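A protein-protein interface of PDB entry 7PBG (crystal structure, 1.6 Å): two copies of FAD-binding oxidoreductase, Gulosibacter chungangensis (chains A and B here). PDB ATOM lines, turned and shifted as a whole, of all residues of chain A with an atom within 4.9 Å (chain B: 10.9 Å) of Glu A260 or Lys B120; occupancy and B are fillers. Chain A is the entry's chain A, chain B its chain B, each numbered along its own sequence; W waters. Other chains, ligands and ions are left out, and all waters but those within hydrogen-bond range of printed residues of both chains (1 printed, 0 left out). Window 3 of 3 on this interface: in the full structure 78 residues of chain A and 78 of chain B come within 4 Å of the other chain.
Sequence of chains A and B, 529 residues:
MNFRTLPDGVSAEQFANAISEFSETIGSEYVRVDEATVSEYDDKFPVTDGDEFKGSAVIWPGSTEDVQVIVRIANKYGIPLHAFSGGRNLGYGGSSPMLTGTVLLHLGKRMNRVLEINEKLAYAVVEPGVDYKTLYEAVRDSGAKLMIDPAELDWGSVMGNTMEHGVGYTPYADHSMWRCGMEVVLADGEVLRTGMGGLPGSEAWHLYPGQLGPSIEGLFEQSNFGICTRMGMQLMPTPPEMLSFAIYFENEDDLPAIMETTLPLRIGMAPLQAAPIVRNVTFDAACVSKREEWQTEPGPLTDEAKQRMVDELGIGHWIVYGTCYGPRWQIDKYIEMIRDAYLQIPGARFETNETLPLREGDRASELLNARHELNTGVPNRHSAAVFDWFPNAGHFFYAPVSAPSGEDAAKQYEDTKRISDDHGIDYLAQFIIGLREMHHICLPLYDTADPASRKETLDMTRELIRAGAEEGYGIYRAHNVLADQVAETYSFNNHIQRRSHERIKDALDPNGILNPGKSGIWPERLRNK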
ATOM      1  N   PRO A 256     -39.569 -38.914  -1.968  1.00  0.00           N
ATOM      2  CA  PRO A 256     -38.275 -38.430  -1.503  1.00  0.00           C
ATOM      3  C   PRO A 256     -37.083 -39.108  -2.181  1.00  0.00           C
ATOM      4  O   PRO A 256     -36.188 -38.420  -2.686  1.00  0.00           O
ATOM      5  CB  PRO A 256     -38.286 -38.706   0.008  1.00  0.00           C
ATOM      6  CG  PRO A 256     -39.724 -38.698   0.347  1.00  0.00           C
ATOM      7  CD  PRO A 256     -40.444 -39.317  -0.848  1.00  0.00           C
ATOM      8  N   ALA A 257     -37.078 -40.435  -2.254  1.00  0.00           N
ATOM      9  CA  ALA A 257     -35.958 -41.115  -2.902  1.00  0.00           C
ATOM     10  C   ALA A 257     -35.876 -40.750  -4.392  1.00  0.00           C
ATOM     11  O   ALA A 257     -34.739 -40.760  -4.969  1.00  0.00           O
ATOM     12  CB  ALA A 257     -36.060 -42.590  -2.720  1.00  0.00           C
ATOM     13  N   ILE A 258     -37.024 -40.607  -5.043  1.00  0.00           N
ATOM     14  CA  ILE A 258     -37.011 -40.233  -6.468  1.00  0.00           C
ATOM     15  C   ILE A 258     -36.272 -38.898  -6.621  1.00  0.00           C
ATOM     16  O   ILE A 258     -35.403 -38.789  -7.461  1.00  0.00           O
ATOM     17  CB  ILE A 258     -38.401 -40.154  -7.071  1.00  0.00           C
ATOM     18  CG1 ILE A 258     -39.119 -41.512  -7.033  1.00  0.00           C
ATOM     19  CG2 ILE A 258     -38.298 -39.520  -8.450  1.00  0.00           C
ATOM     20  CD1 ILE A 258     -40.631 -41.421  -7.304  1.00  0.00           C
ATOM     21  N   MET A 259     -36.615 -37.897  -5.803  1.00  0.00           N
ATOM     22  CA  MET A 259     -36.058 -36.561  -5.993  1.00  0.00           C
ATOM     23  C   MET A 259     -34.561 -36.605  -5.621  1.00  0.00           C
ATOM     24  O   MET A 259     -33.766 -36.011  -6.339  1.00  0.00           O
ATOM     25  CB  MET A 259     -36.807 -35.514  -5.156  1.00  0.00           C
ATOM     26  CG  MET A 259     -38.267 -35.385  -5.454  1.00  0.00           C
ATOM     27  SD  MET A 259     -38.742 -35.306  -7.195  1.00  0.00           S
ATOM     28  CE  MET A 259     -37.907 -33.783  -7.631  1.00  0.00           C
ATOM     29  N   GLU A 260     -34.185 -37.329  -4.550  1.00  0.00           N
ATOM     30  CA  GLU A 260     -32.794 -37.347  -4.084  1.00  0.00           C
ATOM     31  C   GLU A 260     -31.957 -38.167  -5.070  1.00  0.00           C
ATOM     32  O   GLU A 260     -30.771 -37.888  -5.159  1.00  0.00           O
ATOM     33  CB  GLU A 260     -32.706 -37.856  -2.661  1.00  0.00           C
ATOM     34  CG  GLU A 260     -33.290 -36.880  -1.673  1.00  0.00           C
ATOM     35  CD  GLU A 260     -32.492 -35.613  -1.406  1.00  0.00           C
ATOM     36  OE1 GLU A 260     -31.307 -35.554  -1.786  1.00  0.00           O
ATOM     37  OE2 GLU A 260     -33.039 -34.707  -0.761  1.00  0.00           O
ATOM     38  N   THR A 261     -32.548 -39.107  -5.817  1.00  0.00           N
ATOM     39  CA  THR A 261     -31.808 -39.855  -6.857  1.00  0.00           C
ATOM     40  C   THR A 261     -31.585 -38.966  -8.092  1.00  0.00           C
ATOM     41  O   THR A 261     -30.491 -39.006  -8.715  1.00  0.00           O
ATOM     42  CB  THR A 261     -32.509 -41.157  -7.256  1.00  0.00           C
ATOM     43  OG1 THR A 261     -32.637 -41.930  -6.063  1.00  0.00           O
ATOM     44  CG2 THR A 261     -31.761 -41.958  -8.300  1.00  0.00           C
ATOM     45  N   THR A 262     -32.571 -38.148  -8.402  1.00  0.00           N
ATOM     46  CA  THR A 262     -32.600 -37.291  -9.610  1.00  0.00           C
ATOM     47  C   THR A 262     -31.488 -36.223  -9.538  1.00  0.00           C
ATOM     48  O   THR A 262     -30.768 -36.044 -10.490  1.00  0.00           O
ATOM     49  CB  THR A 262     -33.973 -36.628  -9.784  1.00  0.00           C
ATOM     50  OG1 THR A 262     -34.991 -37.630  -9.881  1.00  0.00           O
ATOM     51  CG2 THR A 262     -33.945 -35.723 -10.988  1.00  0.00           C
ATOM     52  N   LEU A 263     -31.347 -35.539  -8.398  1.00  0.00           N
ATOM     53  CA  LEU A 263     -30.513 -34.332  -8.291  1.00  0.00           C
ATOM     54  C   LEU A 263     -29.103 -34.653  -8.795  1.00  0.00           C
ATOM     55  O   LEU A 263     -28.601 -33.946  -9.653  1.00  0.00           O
ATOM     56  CB  LEU A 263     -30.496 -33.851  -6.836  1.00  0.00           C
ATOM     57  CG  LEU A 263     -29.540 -32.701  -6.568  1.00  0.00           C
ATOM     58  CD1 LEU A 263     -29.920 -31.467  -7.352  1.00  0.00           C
ATOM     59  CD2 LEU A 263     -29.500 -32.414  -5.089  1.00  0.00           C
ATOM     60  N   PRO A 264     -28.368 -35.639  -8.234  1.00  0.00           N
ATOM     61  CA  PRO A 264     -26.972 -35.838  -8.627  1.00  0.00           C
ATOM     62  C   PRO A 264     -26.820 -36.305 -10.083  1.00  0.00           C
ATOM     63  O   PRO A 264     -25.730 -36.101 -10.620  1.00  0.00           O
ATOM     64  CB  PRO A 264     -26.440 -36.881  -7.634  1.00  0.00           C
ATOM     65  CG  PRO A 264     -27.689 -37.591  -7.170  1.00  0.00           C
ATOM     66  CD  PRO A 264     -28.713 -36.484  -7.083  1.00  0.00           C
ATOM     67  N   ILE A 267     -27.545 -32.551 -11.985  1.00  0.00           N
ATOM     68  CA  ILE A 267     -26.925 -31.233 -11.701  1.00  0.00           C
ATOM     69  C   ILE A 267     -25.732 -31.005 -12.659  1.00  0.00           C
ATOM     70  O   ILE A 267     -25.408 -29.859 -12.899  1.00  0.00           O
ATOM     71  CB  ILE A 267     -26.528 -31.161 -10.215  1.00  0.00           C
ATOM     72  CG1 ILE A 267     -26.155 -29.729  -9.845  1.00  0.00           C
ATOM     73  CG2 ILE A 267     -25.436 -32.159  -9.886  1.00  0.00           C
ATOM     74  CD1 ILE A 267     -26.270 -29.411  -8.383  1.00  0.00           C
ATOM     75  N   PRO A 404     -33.824 -28.356  -3.868  1.00  0.00           N
ATOM     76  CA  PRO A 404     -34.036 -29.789  -3.981  1.00  0.00           C
ATOM     77  C   PRO A 404     -33.879 -30.522  -2.654  1.00  0.00           C
ATOM     78  O   PRO A 404     -32.872 -30.358  -1.906  1.00  0.00           O
ATOM     79  CB  PRO A 404     -32.982 -30.226  -4.974  1.00  0.00           C
ATOM     80  CG  PRO A 404     -32.825 -29.008  -5.851  1.00  0.00           C
ATOM     81  CD  PRO A 404     -32.847 -27.871  -4.851  1.00  0.00           C
ATOM     82  N   SER A 405     -34.880 -31.345  -2.394  1.00  0.00           N
ATOM     83  CA  SER A 405     -35.043 -32.025  -1.099  1.00  0.00           C
ATOM     84  C   SER A 405     -36.154 -33.037  -1.255  1.00  0.00           C
ATOM     85  O   SER A 405     -37.282 -32.621  -1.511  1.00  0.00           O
ATOM     86  CB  SER A 405     -35.357 -31.072   0.025  1.00  0.00           C
ATOM     87  OG  SER A 405     -35.797 -31.811   1.172  1.00  0.00           O
ATOM     88  N   GLY A 406     -35.832 -34.319  -1.109  1.00  0.00           N
ATOM     89  CA  GLY A 406     -36.870 -35.345  -1.083  1.00  0.00           C
ATOM     90  C   GLY A 406     -37.858 -35.077   0.037  1.00  0.00           C
ATOM     91  O   GLY A 406     -39.059 -35.177  -0.181  1.00  0.00           O
ATOM     92  N   GLU A 407     -37.337 -34.824   1.240  1.00  0.00           N
ATOM     93  CA  GLU A 407     -38.172 -34.726   2.444  1.00  0.00           C
ATOM     94  C   GLU A 407     -39.131 -33.553   2.227  1.00  0.00           C
ATOM     95  O   GLU A 407     -40.353 -33.715   2.494  1.00  0.00           O
ATOM     96  CB  GLU A 407     -37.261 -34.598   3.667  1.00  0.00           C
ATOM     97  CG  GLU A 407     -38.005 -34.268   4.936  1.00  0.00           C
ATOM     98  CD  GLU A 407     -37.093 -33.853   6.075  1.00  0.00           C
ATOM     99  OE1 GLU A 407     -35.930 -34.273   6.070  1.00  0.00           O
ATOM    100  OE2 GLU A 407     -37.544 -33.069   6.945  1.00  0.00           O
ATOM    101  N   GLU B 116     -20.264 -18.925   1.488  1.00  0.00           N
ATOM    102  CA  GLU B 116     -20.911 -20.248   1.452  1.00  0.00           C
ATOM    103  C   GLU B 116     -20.363 -21.026   0.270  1.00  0.00           C
ATOM    104  O   GLU B 116     -20.185 -20.425  -0.792  1.00  0.00           O
ATOM    105  CB  GLU B 116     -22.428 -20.071   1.371  1.00  0.00           C
ATOM    106  CG  GLU B 116     -23.127 -21.405   1.421  1.00  0.00           C
ATOM    107  CD  GLU B 116     -24.638 -21.328   1.367  1.00  0.00           C
ATOM    108  OE1 GLU B 116     -25.195 -20.196   1.517  1.00  0.00           O
ATOM    109  OE2 GLU B 116     -25.240 -22.392   1.085  1.00  0.00           O
ATOM    110  N   ILE B 117     -20.108 -22.313   0.479  1.00  0.00           N
ATOM    111  CA  ILE B 117     -19.895 -23.276  -0.616  1.00  0.00           C
ATOM    112  C   ILE B 117     -20.922 -24.365  -0.376  1.00  0.00           C
ATOM    113  O   ILE B 117     -21.000 -24.886   0.762  1.00  0.00           O
ATOM    114  CB  ILE B 117     -18.457 -23.801  -0.643  1.00  0.00           C
ATOM    115  CG1 ILE B 117     -17.477 -22.665  -0.930  1.00  0.00           C
ATOM    116  CG2 ILE B 117     -18.358 -24.945  -1.645  1.00  0.00           C
ATOM    117  CD1 ILE B 117     -16.068 -22.955  -0.511  1.00  0.00           C
ATOM    118  N   ASN B 118     -21.727 -24.653  -1.389  1.00  0.00           N
ATOM    119  CA  ASN B 118     -22.722 -25.724  -1.289  1.00  0.00           C
ATOM    120  C   ASN B 118     -22.338 -26.773  -2.315  1.00  0.00           C
ATOM    121  O   ASN B 118     -22.516 -26.540  -3.534  1.00  0.00           O
ATOM    122  CB  ASN B 118     -24.115 -25.121  -1.427  1.00  0.00           C
ATOM    123  CG  ASN B 118     -25.201 -26.121  -1.141  1.00  0.00           C
ATOM    124  OD1 ASN B 118     -25.079 -27.282  -1.536  1.00  0.00           O
ATOM    125  ND2 ASN B 118     -26.248 -25.678  -0.471  1.00  0.00           N
ATOM    126  N   GLU B 119     -21.952 -27.958  -1.854  1.00  0.00           N
ATOM    127  CA  GLU B 119     -21.548 -29.019  -2.797  1.00  0.00           C
ATOM    128  C   GLU B 119     -22.779 -29.661  -3.464  1.00  0.00           C
ATOM    129  O   GLU B 119     -22.812 -29.840  -4.703  1.00  0.00           O
ATOM    130  CB  GLU B 119     -20.739 -30.076  -2.066  1.00  0.00           C
ATOM    131  CG  GLU B 119     -20.304 -31.151  -3.012  1.00  0.00           C
ATOM    132  CD  GLU B 119     -19.421 -32.211  -2.417  1.00  0.00           C
ATOM    133  OE1 GLU B 119     -19.641 -32.535  -1.221  1.00  0.00           O
ATOM    134  OE2 GLU B 119     -18.534 -32.702  -3.156  1.00  0.00           O
ATOM    135  N   LYS B 120     -23.780 -30.006  -2.655  1.00  0.00           N
ATOM    136  CA  LYS B 120     -24.981 -30.728  -3.136  1.00  0.00           C
ATOM    137  C   LYS B 120     -25.654 -29.926  -4.265  1.00  0.00           C
ATOM    138  O   LYS B 120     -26.172 -30.530  -5.251  1.00  0.00           O
ATOM    139  CB  LYS B 120     -25.915 -30.912  -1.946  1.00  0.00           C
ATOM    140  CG  LYS B 120     -27.182 -31.673  -2.275  1.00  0.00           C
ATOM    141  CD  LYS B 120     -28.021 -32.056  -1.097  1.00  0.00           C
ATOM    142  CE  LYS B 120     -29.139 -32.969  -1.570  1.00  0.00           C
ATOM    143  NZ  LYS B 120     -30.058 -33.332  -0.457  1.00  0.00           N
ATOM    144  N   LEU B 121     -25.748 -28.593  -4.108  1.00  0.00           N
ATOM    145  CA  LEU B 121     -26.420 -27.738  -5.111  1.00  0.00           C
ATOM    146  C   LEU B 121     -25.419 -26.915  -5.951  1.00  0.00           C
ATOM    147  O   LEU B 121     -25.882 -26.043  -6.750  1.00  0.00           O
ATOM    148  CB  LEU B 121     -27.440 -26.858  -4.384  1.00  0.00           C
ATOM    149  CG  LEU B 121     -28.491 -27.639  -3.603  1.00  0.00           C
ATOM    150  CD1 LEU B 121     -29.475 -26.704  -2.934  1.00  0.00           C
ATOM    151  CD2 LEU B 121     -29.223 -28.628  -4.502  1.00  0.00           C
ATOM    152  N   ALA B 122     -24.114 -27.171  -5.785  1.00  0.00           N
ATOM    153  CA  ALA B 122     -23.017 -26.711  -6.669  1.00  0.00           C
ATOM    154  C   ALA B 122     -23.085 -25.188  -6.856  1.00  0.00           C
ATOM    155  O   ALA B 122     -23.326 -24.696  -7.998  1.00  0.00           O
ATOM    156  CB  ALA B 122     -23.107 -27.429  -7.988  1.00  0.00           C
ATOM    157  N   TYR B 123     -22.855 -24.455  -5.779  1.00  0.00           N
ATOM    158  CA  TYR B 123     -22.761 -22.997  -5.870  1.00  0.00           C
ATOM    159  C   TYR B 123     -21.934 -22.471  -4.700  1.00  0.00           C
ATOM    160  O   TYR B 123     -21.727 -23.209  -3.726  1.00  0.00           O
ATOM    161  CB  TYR B 123     -24.133 -22.340  -5.902  1.00  0.00           C
ATOM    162  CG  TYR B 123     -24.915 -22.340  -4.623  1.00  0.00           C
ATOM    163  CD1 TYR B 123     -24.656 -21.406  -3.632  1.00  0.00           C
ATOM    164  CD2 TYR B 123     -25.874 -23.314  -4.370  1.00  0.00           C
ATOM    165  CE1 TYR B 123     -25.377 -21.389  -2.458  1.00  0.00           C
ATOM    166  CE2 TYR B 123     -26.595 -23.312  -3.202  1.00  0.00           C
ATOM    167  CZ  TYR B 123     -26.343 -22.356  -2.237  1.00  0.00           C
ATOM    168  OH  TYR B 123     -27.060 -22.380  -1.085  1.00  0.00           O
ATOM    169  N   ALA B 124     -21.390 -21.290  -4.921  1.00  0.00           N
ATOM    170  CA  ALA B 124     -20.677 -20.504  -3.897  1.00  0.00           C
ATOM    171  C   ALA B 124     -21.372 -19.152  -3.816  1.00  0.00           C
ATOM    172  O   ALA B 124     -22.111 -18.766  -4.738  1.00  0.00           O
ATOM    173  CB  ALA B 124     -19.234 -20.391  -4.252  1.00  0.00           C
ATOM    174  N   VAL B 139     -12.682 -23.518  -2.389  1.00  0.00           N
ATOM    175  CA  VAL B 139     -13.415 -24.734  -2.839  1.00  0.00           C
ATOM    176  C   VAL B 139     -12.521 -25.956  -2.602  1.00  0.00           C
ATOM    177  O   VAL B 139     -13.025 -27.020  -2.159  1.00  0.00           O
ATOM    178  CB  VAL B 139     -13.843 -24.624  -4.317  1.00  0.00           C
ATOM    179  CG1 VAL B 139     -14.350 -25.940  -4.850  1.00  0.00           C
ATOM    180  CG2 VAL B 139     -14.885 -23.535  -4.490  1.00  0.00           C
ATOM    181  N   SER B 142     -12.688 -26.820   1.045  1.00  0.00           N
ATOM    182  CA  SER B 142     -14.050 -27.323   1.389  1.00  0.00           C
ATOM    183  C   SER B 142     -14.130 -28.828   1.093  1.00  0.00           C
ATOM    184  O   SER B 142     -15.003 -29.481   1.676  1.00  0.00           O
ATOM    185  CB  SER B 142     -15.131 -26.598   0.643  1.00  0.00           C
ATOM    186  OG  SER B 142     -15.177 -27.039  -0.695  1.00  0.00           O
ATOM    187  N   GLY B 143     -13.264 -29.331   0.220  1.00  0.00           N
ATOM    188  CA  GLY B 143     -13.316 -30.698  -0.335  1.00  0.00           C
ATOM    189  C   GLY B 143     -14.483 -30.898  -1.294  1.00  0.00           C
ATOM    190  O   GLY B 143     -14.595 -32.002  -1.799  1.00  0.00           O
ATOM    191  N   ALA B 144     -15.327 -29.891  -1.540  1.00  0.00           N
ATOM    192  CA  ALA B 144     -16.438 -29.980  -2.525  1.00  0.00           C
ATOM    193  C   ALA B 144     -15.890 -30.343  -3.907  1.00  0.00           C
ATOM    194  O   ALA B 144     -14.856 -29.776  -4.336  1.00  0.00           O
ATOM    195  CB  ALA B 144     -17.239 -28.692  -2.556  1.00  0.00           C
ATOM    196  N   LYS B 145     -16.609 -31.197  -4.635  1.00  0.00           N
ATOM    197  CA  LYS B 145     -16.163 -31.647  -5.963  1.00  0.00           C
ATOM    198  C   LYS B 145     -16.757 -30.675  -6.970  1.00  0.00           C
ATOM    199  O   LYS B 145     -17.654 -31.058  -7.740  1.00  0.00           O
ATOM    200  CB  LYS B 145     -16.501 -33.118  -6.167  1.00  0.00           C
ATOM    201  CG  LYS B 145     -15.650 -34.089  -5.360  1.00  0.00           C
ATOM    202  CD  LYS B 145     -14.141 -33.883  -5.451  1.00  0.00           C
ATOM    203  CE  LYS B 145     -13.336 -34.762  -4.508  1.00  0.00           C
ATOM    204  NZ  LYS B 145     -13.143 -34.118  -3.183  1.00  0.00           N
ATOM    205  N   LEU B 146     -16.310 -29.428  -6.900  1.00  0.00           N
ATOM    206  CA  LEU B 146     -16.801 -28.337  -7.781  1.00  0.00           C
ATOM    207  C   LEU B 146     -15.607 -27.668  -8.455  1.00  0.00           C
ATOM    208  O   LEU B 146     -14.511 -27.582  -7.852  1.00  0.00           O
ATOM    209  CB  LEU B 146     -17.553 -27.306  -6.950  1.00  0.00           C
ATOM    210  CG  LEU B 146     -18.758 -27.795  -6.134  1.00  0.00           C
ATOM    211  CD1 LEU B 146     -19.330 -26.630  -5.311  1.00  0.00           C
ATOM    212  CD2 LEU B 146     -19.810 -28.407  -7.051  1.00  0.00           C
ATOM    213  N   TYR B 172     -18.666 -23.474 -18.219  1.00  0.00           N
ATOM    214  CA  TYR B 172     -19.313 -22.396 -17.441  1.00  0.00           C
ATOM    215  C   TYR B 172     -18.696 -21.038 -17.781  1.00  0.00           C
ATOM    216  O   TYR B 172     -18.711 -20.159 -16.889  1.00  0.00           O
ATOM    217  CB  TYR B 172     -19.237 -22.688 -15.943  1.00  0.00           C
ATOM    218  CG  TYR B 172     -20.327 -23.571 -15.377  1.00  0.00           C
ATOM    219  CD1 TYR B 172     -20.758 -24.731 -16.032  1.00  0.00           C
ATOM    220  CD2 TYR B 172     -21.002 -23.225 -14.212  1.00  0.00           C
ATOM    221  CE1 TYR B 172     -21.773 -25.530 -15.506  1.00  0.00           C
ATOM    222  CE2 TYR B 172     -22.028 -24.001 -13.687  1.00  0.00           C
ATOM    223  CZ  TYR B 172     -22.408 -25.178 -14.325  1.00  0.00           C
ATOM    224  OH  TYR B 172     -23.453 -25.913 -13.836  1.00  0.00           O
ATOM    225  N   GLU B 203     -34.591 -20.719   0.189  1.00  0.00           N
ATOM    226  CA  GLU B 203     -33.246 -21.318  -0.005  1.00  0.00           C
ATOM    227  C   GLU B 203     -32.866 -21.294  -1.484  1.00  0.00           C
ATOM    228  O   GLU B 203     -31.819 -21.879  -1.807  1.00  0.00           O
ATOM    229  CB  GLU B 203     -33.243 -22.732   0.565  1.00  0.00           C
ATOM    230  CG  GLU B 203     -33.689 -22.779   2.003  1.00  0.00           C
ATOM    231  CD  GLU B 203     -33.548 -24.167   2.620  1.00  0.00           C
ATOM    232  OE1 GLU B 203     -33.983 -25.148   1.980  1.00  0.00           O
ATOM    233  OE2 GLU B 203     -33.076 -24.258   3.760  1.00  0.00           O
ATOM    234  N   HIS B 206     -29.830 -18.554  -4.735  1.00  0.00           N
ATOM    235  CA  HIS B 206     -28.657 -18.847  -5.579  1.00  0.00           C
ATOM    236  C   HIS B 206     -28.903 -20.046  -6.482  1.00  0.00           C
ATOM    237  O   HIS B 206     -27.955 -20.529  -7.064  1.00  0.00           O
ATOM    238  CB  HIS B 206     -27.408 -19.001  -4.729  1.00  0.00           C
ATOM    239  CG  HIS B 206     -27.222 -17.839  -3.815  1.00  0.00           C
ATOM    240  ND1 HIS B 206     -27.204 -16.514  -4.287  1.00  0.00           N
ATOM    241  CD2 HIS B 206     -27.054 -17.779  -2.476  1.00  0.00           C
ATOM    242  CE1 HIS B 206     -27.051 -15.703  -3.240  1.00  0.00           C
ATOM    243  NE2 HIS B 206     -26.937 -16.459  -2.117  1.00  0.00           N
ATOM    244  N   LEU B 207     -30.146 -20.485  -6.587  1.00  0.00           N
ATOM    245  CA  LEU B 207     -30.541 -21.685  -7.361  1.00  0.00           C
ATOM    246  C   LEU B 207     -31.314 -21.269  -8.580  1.00  0.00           C
ATOM    247  O   LEU B 207     -31.104 -21.879  -9.613  1.00  0.00           O
ATOM    248  CB  LEU B 207     -31.381 -22.652  -6.520  1.00  0.00           C
ATOM    249  CG  LEU B 207     -30.823 -23.045  -5.152  1.00  0.00           C
ATOM    250  CD1 LEU B 207     -31.791 -23.985  -4.450  1.00  0.00           C
ATOM    251  CD2 LEU B 207     -29.460 -23.715  -5.351  1.00  0.00           C
ATOM    252  N   GLN B 234     -22.877 -20.083  -9.512  1.00  0.00           N
ATOM    253  CA  GLN B 234     -23.094 -21.533  -9.602  1.00  0.00           C
ATOM    254  C   GLN B 234     -21.836 -22.143 -10.196  1.00  0.00           C
ATOM    255  O   GLN B 234     -21.217 -21.503 -11.054  1.00  0.00           O
ATOM    256  CB  GLN B 234     -24.350 -21.813 -10.439  1.00  0.00           C
ATOM    257  CG  GLN B 234     -25.588 -21.151  -9.779  1.00  0.00           C
ATOM    258  CD  GLN B 234     -26.859 -21.347 -10.552  1.00  0.00           C
ATOM    259  OE1 GLN B 234     -26.834 -21.575 -11.767  1.00  0.00           O
ATOM    260  NE2 GLN B 234     -28.003 -21.207  -9.877  1.00  0.00           N
ATOM    261  N   LEU B 235     -21.477 -23.316  -9.710  1.00  0.00           N
ATOM    262  CA  LEU B 235     -20.146 -23.916 -10.014  1.00  0.00           C
ATOM    263  C   LEU B 235     -20.366 -25.256 -10.668  1.00  0.00           C
ATOM    264  O   LEU B 235     -21.152 -26.029 -10.167  1.00  0.00           O
ATOM    265  CB  LEU B 235     -19.290 -24.086  -8.758  1.00  0.00           C
ATOM    266  CG  LEU B 235     -18.987 -22.801  -8.005  1.00  0.00           C
ATOM    267  CD1 LEU B 235     -18.179 -23.099  -6.741  1.00  0.00           C
ATOM    268  CD2 LEU B 235     -18.297 -21.767  -8.899  1.00  0.00           C
ATOM    269  N   MET B 236     -19.607 -25.516 -11.718  1.00  0.00           N
ATOM    270  CA  MET B 236     -19.719 -26.782 -12.465  1.00  0.00           C
ATOM    271  C   MET B 236     -19.269 -27.920 -11.562  1.00  0.00           C
ATOM    272  O   MET B 236     -18.190 -27.865 -10.977  1.00  0.00           O
ATOM    273  CB  MET B 236     -18.845 -26.734 -13.704  1.00  0.00           C
ATOM    274  CG  MET B 236     -18.922 -27.970 -14.529  1.00  0.00           C
ATOM    275  SD  MET B 236     -18.115 -27.727 -16.130  1.00  0.00           S
ATOM    276  CE  MET B 236     -17.238 -29.277 -16.332  1.00  0.00           C
ATOM    277  N   PRO B 237     -20.073 -28.983 -11.415  1.00  0.00           N
ATOM    278  CA  PRO B 237     -19.587 -30.207 -10.793  1.00  0.00           C
ATOM    279  C   PRO B 237     -18.383 -30.771 -11.553  1.00  0.00           C
ATOM    280  O   PRO B 237     -18.341 -30.824 -12.769  1.00  0.00           O
ATOM    281  CB  PRO B 237     -20.765 -31.173 -10.795  1.00  0.00           C
ATOM    282  CG  PRO B 237     -21.967 -30.286 -10.972  1.00  0.00           C
ATOM    283  CD  PRO B 237     -21.500 -29.083 -11.781  1.00  0.00           C
ATOM    284  N   THR B 238     -17.382 -31.149 -10.774  1.00  0.00           N
ATOM    285  CA  THR B 238     -16.119 -31.722 -11.332  1.00  0.00           C
ATOM    286  C   THR B 238     -16.454 -33.006 -12.073  1.00  0.00           C
ATOM    287  O   THR B 238     -17.035 -33.949 -11.509  1.00  0.00           O
ATOM    288  CB  THR B 238     -15.055 -31.977 -10.261  1.00  0.00           C
ATOM    289  OG1 THR B 238     -14.895 -30.751  -9.559  1.00  0.00           O
ATOM    290  CG2 THR B 238     -13.724 -32.386 -10.854  1.00  0.00           C
HETATM  291  O   HOH W   1     -23.874 -28.405 -14.716  1.00  0.00           O
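The side-chain amino group (NZ) of Lys B120 is in salt-bridge range of the side-chain carboxylate (OE1) of Glu A260 (2.9 Å).
The backbone carbonyl oxygen of Ala B122 is in hydrogen-bond range of the backbone NH of Leu B235, at 2.9 Å.
The side-chain carboxylate (OE2) of Glu A260 is in hydrogen-bond range of the backbone NH (N) of Gly A406 (2.8 Å).
The backbone NH (N) of Leu B121 is in hydrogen-bond range of the side-chain amide oxygen (OD1) of Asn B118 (3.0 Å).
The side-chain amide oxygen (OD1) of Asn B118 sits at hydrogen-bond distance from the backbone NH (N) of Lys B120 (3.2 Å).
Leu A263 touches Lys B120 (CD2 to CE, 3.6 Å).
CD2 of Leu B121 touches CD2 of Leu A263, at 3.8 Å.
O of Lys B120 touches CD1 of Ile A267 (3.3 Å).
CD1 of Ile A267 touches C of Leu B121 (3.6 Å).
Ile A267 touches Ala B122 (CD1 to CB, 3.8 Å).
CG of Pro B237 touches O of Ile A267, at 3.97 Å.
CD2 of Leu B121 touches CD of Pro A404, at 3.7 Å.
Glu A260 touches just one residue of chain B: Lys B120.
Lys B120 touches just these residues of chain A: Glu A260 (2.9 Å), Leu A263 (3.6 Å) and Ile A267 (3.3 Å).
No residue of chain B comes within 4 Å of Ala A257.
No residue of chain B comes within 4 Å of Met A259.
No residue of chain B comes within 4 Å of Thr A261.
Of chain B, only Lys B120 and Leu B121 come within 4 Å of Leu A263.
No residue of chain B comes within 4 Å of Ser A405.
Gly A406 touches none of the printed residues of chain B.
Of the printed residues of chain A, Leu B121 touches Leu A263, Ile A267 and Pro A404.
Of the printed residues of chain A, Pro B237 touches Ile A267.
Ala B144 touches none of the printed residues of chain A.
The nearest residue of chain A that does not touch Lys B120 is Pro A404 (4.3 Å).
Printed residues of chain B that touch a printed residue of chain A: Lys B120, Leu B121, Ala B122 and Pro B237.
Of the 14 printed residues of chain A, 4 touch a printed residue of chain B.
Printed residues of chain A that touch a printed residue of chain B: Glu A260, Leu A263, Ile A267 and Pro A404.
Among the printed residues, Asp or Glu carboxylates within 4 Å of a Lys or Arg side-chain nitrogen of the other chain: Glu A260 with Lys B120 (2.9 Å).
No position is printed for both chains.
Water W1 lies within hydrogen-bond range of the side-chain hydroxyl of Tyr B172 and the backbone carbonyl oxygen of Ile A267.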
